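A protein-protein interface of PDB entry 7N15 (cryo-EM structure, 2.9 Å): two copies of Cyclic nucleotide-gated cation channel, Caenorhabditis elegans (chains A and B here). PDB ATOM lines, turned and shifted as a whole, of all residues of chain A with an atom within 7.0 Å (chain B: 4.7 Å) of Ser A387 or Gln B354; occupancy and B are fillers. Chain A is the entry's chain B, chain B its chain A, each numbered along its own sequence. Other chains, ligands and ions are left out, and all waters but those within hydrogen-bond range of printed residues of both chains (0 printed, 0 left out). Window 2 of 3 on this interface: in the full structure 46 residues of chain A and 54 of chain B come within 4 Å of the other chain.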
ATOM      1  N   ASP A 344      -5.807   0.408  34.923  1.00  0.00           N
ATOM      2  CA  ASP A 344      -4.576   0.231  34.167  1.00  0.00           C
ATOM      3  C   ASP A 344      -3.424   0.823  34.960  1.00  0.00           C
ATOM      4  O   ASP A 344      -3.584   1.247  36.105  1.00  0.00           O
ATOM      5  CB  ASP A 344      -4.659   0.862  32.779  1.00  0.00           C
ATOM      6  CG  ASP A 344      -5.049   2.305  32.824  1.00  0.00           C
ATOM      7  OD1 ASP A 344      -5.971   2.642  33.577  1.00  0.00           O
ATOM      8  OD2 ASP A 344      -4.419   3.105  32.121  1.00  0.00           O
ATOM      9  N   ALA A 345      -2.251   0.844  34.326  1.00  0.00           N
ATOM     10  CA  ALA A 345      -1.022   1.188  35.029  1.00  0.00           C
ATOM     11  C   ALA A 345      -0.724   2.680  35.032  1.00  0.00           C
ATOM     12  O   ALA A 345       0.259   3.088  35.647  1.00  0.00           O
ATOM     13  CB  ALA A 345       0.153   0.435  34.418  1.00  0.00           C
ATOM     14  N   TRP A 346      -1.525   3.499  34.354  1.00  0.00           N
ATOM     15  CA  TRP A 346      -1.334   4.943  34.417  1.00  0.00           C
ATOM     16  C   TRP A 346      -2.183   5.563  35.512  1.00  0.00           C
ATOM     17  O   TRP A 346      -1.725   6.459  36.230  1.00  0.00           O
ATOM     18  CB  TRP A 346      -1.676   5.571  33.072  1.00  0.00           C
ATOM     19  CG  TRP A 346      -1.578   7.058  33.033  1.00  0.00           C
ATOM     20  CD1 TRP A 346      -0.474   7.788  32.767  1.00  0.00           C
ATOM     21  CD2 TRP A 346      -2.638   7.997  33.243  1.00  0.00           C
ATOM     22  NE1 TRP A 346      -0.768   9.120  32.809  1.00  0.00           N
ATOM     23  CE2 TRP A 346      -2.096   9.273  33.099  1.00  0.00           C
ATOM     24  CE3 TRP A 346      -3.992   7.876  33.555  1.00  0.00           C
ATOM     25  CZ2 TRP A 346      -2.857  10.421  33.252  1.00  0.00           C
ATOM     26  CZ3 TRP A 346      -4.743   9.009  33.704  1.00  0.00           C
ATOM     27  CH2 TRP A 346      -4.176  10.266  33.556  1.00  0.00           C
ATOM     28  N   VAL A 347      -3.428   5.106  35.620  1.00  0.00           N
ATOM     29  CA  VAL A 347      -4.364   5.540  36.643  1.00  0.00           C
ATOM     30  C   VAL A 347      -3.852   5.113  38.020  1.00  0.00           C
ATOM     31  O   VAL A 347      -3.170   4.085  38.145  1.00  0.00           O
ATOM     32  CB  VAL A 347      -5.734   4.924  36.282  1.00  0.00           C
ATOM     33  CG1 VAL A 347      -6.720   5.019  37.357  1.00  0.00           C
ATOM     34  CG2 VAL A 347      -6.310   5.606  35.087  1.00  0.00           C
ATOM     35  N   GLY A 383       8.924  13.772  33.987  1.00  0.00           N
ATOM     36  CA  GLY A 383       8.233  12.693  33.324  1.00  0.00           C
ATOM     37  C   GLY A 383       8.559  11.305  33.809  1.00  0.00           C
ATOM     38  O   GLY A 383       8.358  10.349  33.057  1.00  0.00           O
ATOM     39  N   VAL A 385       7.055   9.111  35.443  1.00  0.00           N
ATOM     40  CA  VAL A 385       5.736   8.625  35.832  1.00  0.00           C
ATOM     41  C   VAL A 385       5.379   7.525  34.845  1.00  0.00           C
ATOM     42  O   VAL A 385       6.048   7.397  33.807  1.00  0.00           O
ATOM     43  CB  VAL A 385       4.695   9.773  35.825  1.00  0.00           C
ATOM     44  CG1 VAL A 385       4.973  10.736  36.942  1.00  0.00           C
ATOM     45  CG2 VAL A 385       4.728  10.490  34.513  1.00  0.00           C
ATOM     46  N   PRO A 386       4.396   6.667  35.158  1.00  0.00           N
ATOM     47  CA  PRO A 386       3.996   5.644  34.187  1.00  0.00           C
ATOM     48  C   PRO A 386       3.383   6.225  32.922  1.00  0.00           C
ATOM     49  O   PRO A 386       2.727   7.267  32.944  1.00  0.00           O
ATOM     50  CB  PRO A 386       2.979   4.811  34.964  1.00  0.00           C
ATOM     51  CG  PRO A 386       3.422   4.909  36.323  1.00  0.00           C
ATOM     52  CD  PRO A 386       3.882   6.311  36.494  1.00  0.00           C
ATOM     53  N   SER A 387       3.640   5.543  31.812  1.00  0.00           N
ATOM     54  CA  SER A 387       3.168   5.972  30.513  1.00  0.00           C
ATOM     55  C   SER A 387       1.657   5.783  30.422  1.00  0.00           C
ATOM     56  O   SER A 387       1.094   4.949  31.135  1.00  0.00           O
ATOM     57  CB  SER A 387       3.866   5.171  29.419  1.00  0.00           C
ATOM     58  OG  SER A 387       5.255   5.428  29.423  1.00  0.00           O
ATOM     59  N   PRO A 388       0.972   6.572  29.586  1.00  0.00           N
ATOM     60  CA  PRO A 388      -0.463   6.361  29.405  1.00  0.00           C
ATOM     61  C   PRO A 388      -0.747   5.061  28.672  1.00  0.00           C
ATOM     62  O   PRO A 388       0.109   4.510  27.979  1.00  0.00           O
ATOM     63  CB  PRO A 388      -0.892   7.572  28.576  1.00  0.00           C
ATOM     64  CG  PRO A 388       0.148   8.566  28.786  1.00  0.00           C
ATOM     65  CD  PRO A 388       1.406   7.810  28.919  1.00  0.00           C
ATOM     66  N   VAL A 389      -1.950   4.542  28.876  1.00  0.00           N
ATOM     67  CA  VAL A 389      -2.398   3.315  28.232  1.00  0.00           C
ATOM     68  C   VAL A 389      -3.512   3.600  27.235  1.00  0.00           C
ATOM     69  O   VAL A 389      -3.354   3.381  26.034  1.00  0.00           O
ATOM     70  CB  VAL A 389      -2.838   2.267  29.277  1.00  0.00           C
ATOM     71  CG1 VAL A 389      -3.215   0.979  28.599  1.00  0.00           C
ATOM     72  CG2 VAL A 389      -1.740   2.033  30.288  1.00  0.00           C
ATOM     73  N   ARG A 390      -4.639   4.108  27.713  1.00  0.00           N
ATOM     74  CA  ARG A 390      -5.762   4.426  26.851  1.00  0.00           C
ATOM     75  C   ARG A 390      -5.527   5.753  26.144  1.00  0.00           C
ATOM     76  O   ARG A 390      -4.685   6.548  26.552  1.00  0.00           O
ATOM     77  CB  ARG A 390      -7.043   4.474  27.674  1.00  0.00           C
ATOM     78  CG  ARG A 390      -7.313   3.187  28.406  1.00  0.00           C
ATOM     79  CD  ARG A 390      -8.278   3.396  29.538  1.00  0.00           C
ATOM     80  NE  ARG A 390      -9.503   4.041  29.093  1.00  0.00           N
ATOM     81  CZ  ARG A 390     -10.587   3.384  28.702  1.00  0.00           C
ATOM     82  NH1 ARG A 390     -10.595   2.061  28.698  1.00  0.00           N
ATOM     83  NH2 ARG A 390     -11.660   4.050  28.311  1.00  0.00           N
ATOM     84  N   GLU A 393      -5.959   9.022  28.109  1.00  0.00           N
ATOM     85  CA  GLU A 393      -4.826   9.323  28.970  1.00  0.00           C
ATOM     86  C   GLU A 393      -3.659   9.872  28.175  1.00  0.00           C
ATOM     87  O   GLU A 393      -2.929  10.726  28.676  1.00  0.00           O
ATOM     88  CB  GLU A 393      -4.407   8.073  29.721  1.00  0.00           C
ATOM     89  CG  GLU A 393      -5.569   7.282  30.205  1.00  0.00           C
ATOM     90  CD  GLU A 393      -5.153   6.030  30.890  1.00  0.00           C
ATOM     91  OE1 GLU A 393      -4.000   5.622  30.702  1.00  0.00           O
ATOM     92  OE2 GLU A 393      -5.976   5.456  31.620  1.00  0.00           O
ATOM     93  N   TYR A 394      -3.489   9.410  26.934  1.00  0.00           N
ATOM     94  CA  TYR A 394      -2.489   9.981  26.037  1.00  0.00           C
ATOM     95  C   TYR A 394      -2.816  11.420  25.684  1.00  0.00           C
ATOM     96  O   TYR A 394      -1.921  12.270  25.656  1.00  0.00           O
ATOM     97  CB  TYR A 394      -2.403   9.159  24.760  1.00  0.00           C
ATOM     98  CG  TYR A 394      -1.440   8.012  24.796  1.00  0.00           C
ATOM     99  CD1 TYR A 394      -1.847   6.764  25.196  1.00  0.00           C
ATOM    100  CD2 TYR A 394      -0.133   8.173  24.404  1.00  0.00           C
ATOM    101  CE1 TYR A 394      -0.976   5.717  25.235  1.00  0.00           C
ATOM    102  CE2 TYR A 394       0.749   7.122  24.430  1.00  0.00           C
ATOM    103  CZ  TYR A 394       0.326   5.900  24.848  1.00  0.00           C
ATOM    104  OH  TYR A 394       1.205   4.849  24.884  1.00  0.00           O
ATOM    105  N   VAL A 397      -2.253  13.538  28.907  1.00  0.00           N
ATOM    106  CA  VAL A 397      -0.843  13.695  29.239  1.00  0.00           C
ATOM    107  C   VAL A 397      -0.132  14.560  28.205  1.00  0.00           C
ATOM    108  O   VAL A 397       0.708  15.383  28.571  1.00  0.00           O
ATOM    109  CB  VAL A 397      -0.216  12.299  29.419  1.00  0.00           C
ATOM    110  CG1 VAL A 397       1.287  12.308  29.340  1.00  0.00           C
ATOM    111  CG2 VAL A 397      -0.591  11.787  30.758  1.00  0.00           C
ATOM    112  N   ASN B 352       6.452  -2.974  20.781  1.00  0.00           N
ATOM    113  CA  ASN B 352       6.762  -1.710  21.433  1.00  0.00           C
ATOM    114  C   ASN B 352       6.314  -1.707  22.888  1.00  0.00           C
ATOM    115  O   ASN B 352       7.078  -1.285  23.766  1.00  0.00           O
ATOM    116  CB  ASN B 352       6.104  -0.569  20.668  1.00  0.00           C
ATOM    117  CG  ASN B 352       6.758   0.760  20.916  1.00  0.00           C
ATOM    118  OD1 ASN B 352       6.697   1.300  22.008  1.00  0.00           O
ATOM    119  ND2 ASN B 352       7.362   1.314  19.887  1.00  0.00           N
ATOM    120  N   LYS B 353       5.049  -2.087  23.135  1.00  0.00           N
ATOM    121  CA  LYS B 353       4.352  -2.255  24.419  1.00  0.00           C
ATOM    122  C   LYS B 353       4.052  -0.943  25.139  1.00  0.00           C
ATOM    123  O   LYS B 353       3.361  -0.944  26.161  1.00  0.00           O
ATOM    124  CB  LYS B 353       5.098  -3.198  25.372  1.00  0.00           C
ATOM    125  CG  LYS B 353       5.286  -4.598  24.849  1.00  0.00           C
ATOM    126  CD  LYS B 353       3.966  -5.314  24.711  1.00  0.00           C
ATOM    127  CE  LYS B 353       4.184  -6.793  24.479  1.00  0.00           C
ATOM    128  NZ  LYS B 353       4.576  -7.093  23.076  1.00  0.00           N
ATOM    129  N   GLN B 354       4.564   0.175  24.631  1.00  0.00           N
ATOM    130  CA  GLN B 354       4.029   1.478  24.986  1.00  0.00           C
ATOM    131  C   GLN B 354       3.009   1.914  23.952  1.00  0.00           C
ATOM    132  O   GLN B 354       1.987   2.520  24.292  1.00  0.00           O
ATOM    133  CB  GLN B 354       5.164   2.495  25.091  1.00  0.00           C
ATOM    134  CG  GLN B 354       4.729   3.905  25.406  1.00  0.00           C
ATOM    135  CD  GLN B 354       5.834   4.734  25.987  1.00  0.00           C
ATOM    136  OE1 GLN B 354       6.957   4.274  26.121  1.00  0.00           O
ATOM    137  NE2 GLN B 354       5.522   5.963  26.340  1.00  0.00           N
ATOM    138  N   SER B 355       3.261   1.569  22.693  1.00  0.00           N
ATOM    139  CA  SER B 355       2.337   1.841  21.606  1.00  0.00           C
ATOM    140  C   SER B 355       1.105   0.962  21.702  1.00  0.00           C
ATOM    141  O   SER B 355      -0.024   1.459  21.677  1.00  0.00           O
ATOM    142  CB  SER B 355       3.036   1.606  20.280  1.00  0.00           C
ATOM    143  OG  SER B 355       2.989   0.244  19.936  1.00  0.00           O
ATOM    144  N   LEU B 356       1.302  -0.349  21.805  1.00  0.00           N
ATOM    145  CA  LEU B 356       0.211  -1.307  21.957  1.00  0.00           C
ATOM    146  C   LEU B 356       0.405  -2.087  23.248  1.00  0.00           C
ATOM    147  O   LEU B 356       1.010  -3.168  23.244  1.00  0.00           O
ATOM    148  CB  LEU B 356       0.139  -2.246  20.759  1.00  0.00           C
ATOM    149  CG  LEU B 356      -0.140  -1.551  19.434  1.00  0.00           C
ATOM    150  CD1 LEU B 356      -0.068  -2.526  18.307  1.00  0.00           C
ATOM    151  CD2 LEU B 356      -1.491  -0.900  19.490  1.00  0.00           C
ATOM    152  N   PRO B 357      -0.107  -1.587  24.377  1.00  0.00           N
ATOM    153  CA  PRO B 357      -0.118  -2.381  25.608  1.00  0.00           C
ATOM    154  C   PRO B 357      -1.198  -3.446  25.611  1.00  0.00           C
ATOM    155  O   PRO B 357      -1.845  -3.710  24.591  1.00  0.00           O
ATOM    156  CB  PRO B 357      -0.383  -1.336  26.699  1.00  0.00           C
ATOM    157  CG  PRO B 357      -0.201  -0.031  26.064  1.00  0.00           C
ATOM    158  CD  PRO B 357      -0.542  -0.212  24.640  1.00  0.00           C
ATOM    159  N   ARG B 366      -5.135   5.117  17.181  1.00  0.00           N
ATOM    160  CA  ARG B 366      -4.038   4.704  18.049  1.00  0.00           C
ATOM    161  C   ARG B 366      -2.685   5.024  17.430  1.00  0.00           C
ATOM    162  O   ARG B 366      -1.762   5.442  18.137  1.00  0.00           O
ATOM    163  CB  ARG B 366      -4.149   3.212  18.345  1.00  0.00           C
ATOM    164  CG  ARG B 366      -3.137   2.683  19.325  1.00  0.00           C
ATOM    165  CD  ARG B 366      -3.215   3.446  20.611  1.00  0.00           C
ATOM    166  NE  ARG B 366      -2.219   3.008  21.570  1.00  0.00           N
ATOM    167  CZ  ARG B 366      -2.234   3.352  22.846  1.00  0.00           C
ATOM    168  NH1 ARG B 366      -3.193   4.132  23.306  1.00  0.00           N
ATOM    169  NH2 ARG B 366      -1.294   2.910  23.655  1.00  0.00           N
ATOM    170  N   TYR B 370      -0.348   7.705  19.338  1.00  0.00           N
ATOM    171  CA  TYR B 370       0.979   7.333  19.810  1.00  0.00           C
ATOM    172  C   TYR B 370       2.082   8.101  19.092  1.00  0.00           C
ATOM    173  O   TYR B 370       3.087   8.442  19.719  1.00  0.00           O
ATOM    174  CB  TYR B 370       1.216   5.833  19.662  1.00  0.00           C
ATOM    175  CG  TYR B 370       2.583   5.437  20.166  1.00  0.00           C
ATOM    176  CD1 TYR B 370       2.882   5.502  21.518  1.00  0.00           C
ATOM    177  CD2 TYR B 370       3.593   5.057  19.286  1.00  0.00           C
ATOM    178  CE1 TYR B 370       4.131   5.174  21.984  1.00  0.00           C
ATOM    179  CE2 TYR B 370       4.845   4.728  19.746  1.00  0.00           C
ATOM    180  CZ  TYR B 370       5.104   4.787  21.094  1.00  0.00           C
ATOM    181  OH  TYR B 370       6.348   4.454  21.558  1.00  0.00           O
ATOM    182  N   TYR B 373       2.154  11.563  20.643  1.00  0.00           N
ATOM    183  CA  TYR B 373       2.752  11.496  21.975  1.00  0.00           C
ATOM    184  C   TYR B 373       4.260  11.286  21.924  1.00  0.00           C
ATOM    185  O   TYR B 373       4.988  11.884  22.728  1.00  0.00           O
ATOM    186  CB  TYR B 373       2.098  10.375  22.765  1.00  0.00           C
ATOM    187  CG  TYR B 373       2.667  10.133  24.143  1.00  0.00           C
ATOM    188  CD1 TYR B 373       2.311  10.944  25.215  1.00  0.00           C
ATOM    189  CD2 TYR B 373       3.541   9.074  24.380  1.00  0.00           C
ATOM    190  CE1 TYR B 373       2.817  10.713  26.471  1.00  0.00           C
ATOM    191  CE2 TYR B 373       4.033   8.832  25.627  1.00  0.00           C
ATOM    192  CZ  TYR B 373       3.679   9.659  26.667  1.00  0.00           C
ATOM    193  OH  TYR B 373       4.194   9.418  27.914  1.00  0.00           O
ATOM    194  N   GLU B 384      10.655   9.873  27.401  1.00  0.00           N
ATOM    195  CA  GLU B 384      10.143   8.674  28.069  1.00  0.00           C
ATOM    196  C   GLU B 384       9.480   7.748  27.048  1.00  0.00           C
ATOM    197  O   GLU B 384       8.325   7.335  27.172  1.00  0.00           O
ATOM    198  CB  GLU B 384       9.184   9.062  29.181  1.00  0.00           C
ATOM    199  CG  GLU B 384       9.766  10.070  30.133  1.00  0.00           C
ATOM    200  CD  GLU B 384      10.694   9.441  31.139  1.00  0.00           C
ATOM    201  OE1 GLU B 384      10.483   8.265  31.490  1.00  0.00           O
ATOM    202  OE2 GLU B 384      11.640  10.125  31.578  1.00  0.00           O
ATOM    203  N   VAL B 385      10.263   7.409  26.031  1.00  0.00           N
ATOM    204  CA  VAL B 385       9.862   6.601  24.885  1.00  0.00           C
ATOM    205  C   VAL B 385      10.859   5.455  24.802  1.00  0.00           C
ATOM    206  O   VAL B 385      11.909   5.512  25.462  1.00  0.00           O
ATOM    207  CB  VAL B 385       9.838   7.447  23.588  1.00  0.00           C
ATOM    208  CG1 VAL B 385       8.712   8.438  23.632  1.00  0.00           C
ATOM    209  CG2 VAL B 385      11.140   8.162  23.415  1.00  0.00           C
ATOM    210  N   PRO B 386      10.543   4.374  24.074  1.00  0.00           N
ATOM    211  CA  PRO B 386      11.522   3.292  23.929  1.00  0.00           C
ATOM    212  C   PRO B 386      12.770   3.711  23.167  1.00  0.00           C
ATOM    213  O   PRO B 386      12.725   4.552  22.269  1.00  0.00           O
ATOM    214  CB  PRO B 386      10.744   2.221  23.169  1.00  0.00           C
ATOM    215  CG  PRO B 386       9.389   2.415  23.597  1.00  0.00           C
ATOM    216  CD  PRO B 386       9.205   3.886  23.690  1.00  0.00           C
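OE1 of Glu B384 lies close to O of Gly A383, at 3.4 Å. NH2 of Arg B366 sits close to OH of Tyr A394 (3.4 Å). NE2 of Gln B354 is in hydrogen-bond range of OG of Ser A387, 3.1 Å away. The side-chain hydroxyl (OH) of Tyr A394 sits at hydrogen-bond distance from the backbone carbonyl oxygen (O) of Gln B354. The backbone carbonyl oxygen of Val A389 lies within hydrogen-bond range of the guanidinium group of Arg B366 (2.8 Å).
NE of Arg B366 lies within hydrogen-bond range of O of Ser B355 (2.7 Å). The backbone NH of Val A389 lies within hydrogen-bond range of the side-chain carboxylate of Glu A393 (3.0 Å). NE2 of Gln B354 sits at hydrogen-bond distance from O of Glu B384 (3.2 Å). The side-chain hydroxyl of Tyr A394 lies close to the backbone carbonyl oxygen of Pro A388 (3.3 Å). The side-chain amide oxygen (OD1) of Asn B352 lies within hydrogen-bond range of the side-chain hydroxyl (OH) of Tyr B370, 3.2 Å away. The backbone carbonyl oxygen (O) of Gln B354 lies within hydrogen-bond range of the guanidinium group (NH2) of Arg B366 (3.4 Å).
Pro A388 touches Tyr B373. Tyr A394 touches Tyr B370. Tyr A394 touches Tyr B373 (CE2 to CD2, 3.4 Å). Val A397 touches Tyr B373.
Ser A387 touches one residue of chain B. Of the printed residues of chain A, Gln B354 touches Ser A387 and Tyr A394. Of the printed residues of chain B, Tyr A394 touches Gln B354 (2.5 Å), Arg B366 (3.2 Å), Tyr B370 (3.8 Å) and Tyr B373 (3.4 Å). Printed residues of chain B within 4 Å of Val A389: Arg B366. Printed residues of chain B within 4 Å of Pro A388: Tyr B373. Of the printed residues of chain A, Arg B366 touches Val A389 (2.8 Å) and Tyr A394 (3.2 Å). Of the printed residues of chain A, Tyr B373 touches Pro A388, Tyr A394 and Val A397. The nearest residue of chain B that does not touch Ser A387 is Glu B384 (4.3 Å).
Of the 12 printed residues of chain B, 5 touch a printed residue of chain A.
Positions printed for both chains: 385 and 386.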
